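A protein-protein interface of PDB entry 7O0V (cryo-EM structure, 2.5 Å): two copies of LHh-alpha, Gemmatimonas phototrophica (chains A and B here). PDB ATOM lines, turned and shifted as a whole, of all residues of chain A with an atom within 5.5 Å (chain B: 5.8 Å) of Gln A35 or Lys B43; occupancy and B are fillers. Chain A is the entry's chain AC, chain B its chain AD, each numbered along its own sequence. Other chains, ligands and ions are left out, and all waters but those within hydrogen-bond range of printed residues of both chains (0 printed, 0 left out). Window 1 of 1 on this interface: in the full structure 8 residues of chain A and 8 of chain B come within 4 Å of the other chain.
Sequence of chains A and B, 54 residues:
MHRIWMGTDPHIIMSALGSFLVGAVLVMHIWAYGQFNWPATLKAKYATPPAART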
ATOM      1  N   TRP A  31       0.546  10.645  25.821  1.00  0.00           N
ATOM      2  CA  TRP A  31      -0.151   9.412  25.470  1.00  0.00           C
ATOM      3  C   TRP A  31       0.201   8.964  24.055  1.00  0.00           C
ATOM      4  O   TRP A  31       0.586   7.811  23.834  1.00  0.00           O
ATOM      5  CB  TRP A  31      -1.662   9.603  25.621  1.00  0.00           C
ATOM      6  CG  TRP A  31      -2.456   8.389  25.245  1.00  0.00           C
ATOM      7  CD1 TRP A  31      -2.802   7.354  26.063  1.00  0.00           C
ATOM      8  CD2 TRP A  31      -3.008   8.085  23.958  1.00  0.00           C
ATOM      9  NE1 TRP A  31      -3.530   6.423  25.365  1.00  0.00           N
ATOM     10  CE2 TRP A  31      -3.672   6.848  24.071  1.00  0.00           C
ATOM     11  CE3 TRP A  31      -3.006   8.737  22.722  1.00  0.00           C
ATOM     12  CZ2 TRP A  31      -4.324   6.250  22.995  1.00  0.00           C
ATOM     13  CZ3 TRP A  31      -3.654   8.142  21.655  1.00  0.00           C
ATOM     14  CH2 TRP A  31      -4.304   6.911  21.799  1.00  0.00           C
ATOM     15  N   ALA A  32       0.067   9.869  23.082  1.00  0.00           N
ATOM     16  CA  ALA A  32       0.295   9.517  21.683  1.00  0.00           C
ATOM     17  C   ALA A  32       1.728   9.060  21.432  1.00  0.00           C
ATOM     18  O   ALA A  32       1.954   8.119  20.662  1.00  0.00           O
ATOM     19  CB  ALA A  32      -0.052  10.702  20.784  1.00  0.00           C
ATOM     20  N   TYR A  33       2.708   9.715  22.060  1.00  0.00           N
ATOM     21  CA  TYR A  33       4.096   9.277  21.917  1.00  0.00           C
ATOM     22  C   TYR A  33       4.285   7.839  22.382  1.00  0.00           C
ATOM     23  O   TYR A  33       5.080   7.090  21.802  1.00  0.00           O
ATOM     24  CB  TYR A  33       5.032  10.189  22.711  1.00  0.00           C
ATOM     25  CG  TYR A  33       5.103  11.635  22.279  1.00  0.00           C
ATOM     26  CD1 TYR A  33       4.697  12.035  21.014  1.00  0.00           C
ATOM     27  CD2 TYR A  33       5.614  12.599  23.136  1.00  0.00           C
ATOM     28  CE1 TYR A  33       4.762  13.363  20.633  1.00  0.00           C
ATOM     29  CE2 TYR A  33       5.699  13.921  22.760  1.00  0.00           C
ATOM     30  CZ  TYR A  33       5.269  14.300  21.510  1.00  0.00           C
ATOM     31  OH  TYR A  33       5.373  15.616  21.129  1.00  0.00           O
ATOM     32  N   GLY A  34       3.565   7.435  23.427  1.00  0.00           N
ATOM     33  CA  GLY A  34       3.638   6.057  23.885  1.00  0.00           C
ATOM     34  C   GLY A  34       3.110   5.046  22.883  1.00  0.00           C
ATOM     35  O   GLY A  34       3.708   3.986  22.685  1.00  0.00           O
ATOM     36  N   GLN A  35       1.989   5.359  22.234  1.00  0.00           N
ATOM     37  CA  GLN A  35       1.383   4.407  21.307  1.00  0.00           C
ATOM     38  C   GLN A  35       2.082   4.382  19.951  1.00  0.00           C
ATOM     39  O   GLN A  35       2.376   3.307  19.420  1.00  0.00           O
ATOM     40  CB  GLN A  35      -0.103   4.731  21.121  1.00  0.00           C
ATOM     41  CG  GLN A  35      -0.886   5.037  22.397  1.00  0.00           C
ATOM     42  CD  GLN A  35      -0.657   4.036  23.518  1.00  0.00           C
ATOM     43  OE1 GLN A  35      -0.406   2.855  23.280  1.00  0.00           O
ATOM     44  NE2 GLN A  35      -0.757   4.508  24.754  1.00  0.00           N
ATOM     45  N   PHE A  36       2.351   5.547  19.371  1.00  0.00           N
ATOM     46  CA  PHE A  36       2.757   5.605  17.971  1.00  0.00           C
ATOM     47  C   PHE A  36       4.223   5.262  17.731  1.00  0.00           C
ATOM     48  O   PHE A  36       4.643   5.233  16.569  1.00  0.00           O
ATOM     49  CB  PHE A  36       2.401   6.972  17.391  1.00  0.00           C
ATOM     50  CG  PHE A  36       0.947   7.096  17.052  1.00  0.00           C
ATOM     51  CD1 PHE A  36       0.016   7.380  18.035  1.00  0.00           C
ATOM     52  CD2 PHE A  36       0.502   6.869  15.761  1.00  0.00           C
ATOM     53  CE1 PHE A  36      -1.327   7.468  17.731  1.00  0.00           C
ATOM     54  CE2 PHE A  36      -0.839   6.957  15.452  1.00  0.00           C
ATOM     55  CZ  PHE A  36      -1.754   7.255  16.438  1.00  0.00           C
ATOM     56  N   ASN A  37       5.007   5.015  18.784  1.00  0.00           N
ATOM     57  CA  ASN A  37       6.451   4.786  18.667  1.00  0.00           C
ATOM     58  C   ASN A  37       7.173   5.955  17.997  1.00  0.00           C
ATOM     59  O   ASN A  37       8.158   5.766  17.281  1.00  0.00           O
ATOM     60  CB  ASN A  37       6.730   3.472  17.927  1.00  0.00           C
ATOM     61  CG  ASN A  37       8.126   2.938  18.176  1.00  0.00           C
ATOM     62  OD1 ASN A  37       8.683   3.107  19.259  1.00  0.00           O
ATOM     63  ND2 ASN A  37       8.690   2.273  17.177  1.00  0.00           N
ATOM     64  N   PRO B  39      -5.702   0.926  22.722  1.00  0.00           N
ATOM     65  CA  PRO B  39      -4.635   1.082  21.726  1.00  0.00           C
ATOM     66  C   PRO B  39      -3.561  -0.008  21.699  1.00  0.00           C
ATOM     67  O   PRO B  39      -2.580   0.160  20.981  1.00  0.00           O
ATOM     68  CB  PRO B  39      -4.000   2.417  22.127  1.00  0.00           C
ATOM     69  CG  PRO B  39      -4.118   2.413  23.600  1.00  0.00           C
ATOM     70  CD  PRO B  39      -5.500   1.853  23.849  1.00  0.00           C
ATOM     71  N   ALA B  40      -3.723  -1.077  22.479  1.00  0.00           N
ATOM     72  CA  ALA B  40      -2.711  -2.131  22.513  1.00  0.00           C
ATOM     73  C   ALA B  40      -2.385  -2.701  21.132  1.00  0.00           C
ATOM     74  O   ALA B  40      -1.211  -2.913  20.811  1.00  0.00           O
ATOM     75  CB  ALA B  40      -3.164  -3.251  23.451  1.00  0.00           C
ATOM     76  N   THR B  41      -3.397  -2.952  20.295  1.00  0.00           N
ATOM     77  CA  THR B  41      -3.106  -3.372  18.923  1.00  0.00           C
ATOM     78  C   THR B  41      -2.466  -2.265  18.093  1.00  0.00           C
ATOM     79  O   THR B  41      -1.643  -2.551  17.216  1.00  0.00           O
ATOM     80  CB  THR B  41      -4.372  -3.875  18.227  1.00  0.00           C
ATOM     81  OG1 THR B  41      -5.374  -2.853  18.232  1.00  0.00           O
ATOM     82  CG2 THR B  41      -4.903  -5.124  18.909  1.00  0.00           C
ATOM     83  N   LEU B  42      -2.829  -1.006  18.343  1.00  0.00           N
ATOM     84  CA  LEU B  42      -2.150   0.114  17.695  1.00  0.00           C
ATOM     85  C   LEU B  42      -0.670   0.156  18.059  1.00  0.00           C
ATOM     86  O   LEU B  42       0.195   0.270  17.183  1.00  0.00           O
ATOM     87  CB  LEU B  42      -2.842   1.425  18.069  1.00  0.00           C
ATOM     88  CG  LEU B  42      -2.057   2.722  17.881  1.00  0.00           C
ATOM     89  CD1 LEU B  42      -1.763   2.966  16.412  1.00  0.00           C
ATOM     90  CD2 LEU B  42      -2.829   3.887  18.469  1.00  0.00           C
ATOM     91  N   LYS B  43      -0.364   0.072  19.354  1.00  0.00           N
ATOM     92  CA  LYS B  43       1.025   0.053  19.802  1.00  0.00           C
ATOM     93  C   LYS B  43       1.795  -1.126  19.216  1.00  0.00           C
ATOM     94  O   LYS B  43       2.944  -0.974  18.788  1.00  0.00           O
ATOM     95  CB  LYS B  43       1.068   0.021  21.329  1.00  0.00           C
ATOM     96  CG  LYS B  43       2.434   0.291  21.927  1.00  0.00           C
ATOM     97  CD  LYS B  43       2.369   0.275  23.444  1.00  0.00           C
ATOM     98  CE  LYS B  43       3.726   0.558  24.058  1.00  0.00           C
ATOM     99  NZ  LYS B  43       3.688   0.457  25.541  1.00  0.00           N
ATOM    100  N   ALA B  44       1.178  -2.308  19.187  1.00  0.00           N
ATOM    101  CA  ALA B  44       1.810  -3.475  18.576  1.00  0.00           C
ATOM    102  C   ALA B  44       2.067  -3.296  17.083  1.00  0.00           C
ATOM    103  O   ALA B  44       3.035  -3.854  16.555  1.00  0.00           O
ATOM    104  CB  ALA B  44       0.951  -4.717  18.815  1.00  0.00           C
ATOM    105  N   LYS B  45       1.219  -2.539  16.385  1.00  0.00           N
ATOM    106  CA  LYS B  45       1.439  -2.296  14.960  1.00  0.00           C
ATOM    107  C   LYS B  45       2.749  -1.557  14.694  1.00  0.00           C
ATOM    108  O   LYS B  45       3.507  -1.928  13.790  1.00  0.00           O
ATOM    109  CB  LYS B  45       0.264  -1.515  14.367  1.00  0.00           C
ATOM    110  CG  LYS B  45       0.257  -1.502  12.842  1.00  0.00           C
ATOM    111  CD  LYS B  45      -0.711  -0.477  12.255  1.00  0.00           C
ATOM    112  CE  LYS B  45      -2.161  -0.798  12.573  1.00  0.00           C
ATOM    113  NZ  LYS B  45      -3.093   0.078  11.807  1.00  0.00           N
ATOM    114  N   TYR B  46       3.031  -0.503  15.459  1.00  0.00           N
ATOM    115  CA  TYR B  46       4.190   0.347  15.202  1.00  0.00           C
ATOM    116  C   TYR B  46       5.394   0.085  16.103  1.00  0.00           C
ATOM    117  O   TYR B  46       6.461   0.653  15.850  1.00  0.00           O
ATOM    118  CB  TYR B  46       3.776   1.820  15.295  1.00  0.00           C
ATOM    119  CG  TYR B  46       2.775   2.186  14.226  1.00  0.00           C
ATOM    120  CD1 TYR B  46       3.110   2.095  12.882  1.00  0.00           C
ATOM    121  CD2 TYR B  46       1.488   2.586  14.555  1.00  0.00           C
ATOM    122  CE1 TYR B  46       2.200   2.412  11.897  1.00  0.00           C
ATOM    123  CE2 TYR B  46       0.569   2.905  13.573  1.00  0.00           C
ATOM    124  CZ  TYR B  46       0.932   2.815  12.246  1.00  0.00           C
ATOM    125  OH  TYR B  46       0.022   3.129  11.263  1.00  0.00           O
ATOM    126  N   ALA B  47       5.258  -0.735  17.142  1.00  0.00           N
ATOM    127  CA  ALA B  47       6.390  -1.066  18.000  1.00  0.00           C
ATOM    128  C   ALA B  47       7.521  -1.732  17.215  1.00  0.00           C
ATOM    129  O   ALA B  47       7.337  -2.245  16.107  1.00  0.00           O
ATOM    130  CB  ALA B  47       5.949  -1.983  19.140  1.00  0.00           C
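The backbone carbonyl oxygen of Tyr B46 lies within hydrogen-bond range of the side-chain amide nitrogen of Asn A37 (3.1 Å).
The indole nitrogen (NE1) of Trp A31 sits close to the side-chain amide nitrogen (NE2) of Gln A35 (3.4 Å).
Pro B39 touches Trp A31. Lys B43 touches Gly A34 (CE to O, 3.7 Å). OE1 of Gln A35 touches CG of Pro B39 (3.8 Å). Leu B42 touches Gln A35. Gln A35 touches Lys B43 (O to CA, 3.5 Å). CE1 of Phe A36 touches CD2 of Leu B42, 3.95 Å away. O of Phe A36 touches CB of Tyr B46, at 3.7 Å.
Of the printed residues of chain B, Trp A31 touches Pro B39 (3.9 Å). Printed residues of chain B within 4 Å of Gly A34: Lys B43. Of chain B, only Pro B39, Leu B42 and Lys B43 come within 4 Å of Gln A35. Printed residues of chain B within 4 Å of Phe A36: Leu B42 and Tyr B46. Of the printed residues of chain A, Leu B42 touches Gln A35 (3.9 Å) and Phe A36 (3.95 Å). Of chain A, only Gly A34 (3.7 Å) and Gln A35 (3.5 Å) come within 4 Å of Lys B43. The nearest residue of chain B that does not touch Gln A35 is Tyr B46 (4.6 Å). The nearest printed residue of chain A that does not touch Lys B43 is Phe A36 (5.7 Å).
Of the 9 printed residues of chain B, 4 touch a printed residue of chain A. Printed residues of chain B that touch a printed residue of chain A: Pro B39, Leu B42, Lys B43 and Tyr B46. Hydrophobic or aromatic side chains of chain B that line the printed part of chain A: Pro B39, Leu B42 and Tyr B46. Among the printed residues, no Asp or Glu carboxylate lies within 4 Å of a Lys or Arg side-chain nitrogen of the other chain.
No position is printed for both chains. Of the 8 pairs that touch across the chains among the printed residues, none has its exchanged pair printed and touching as well.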
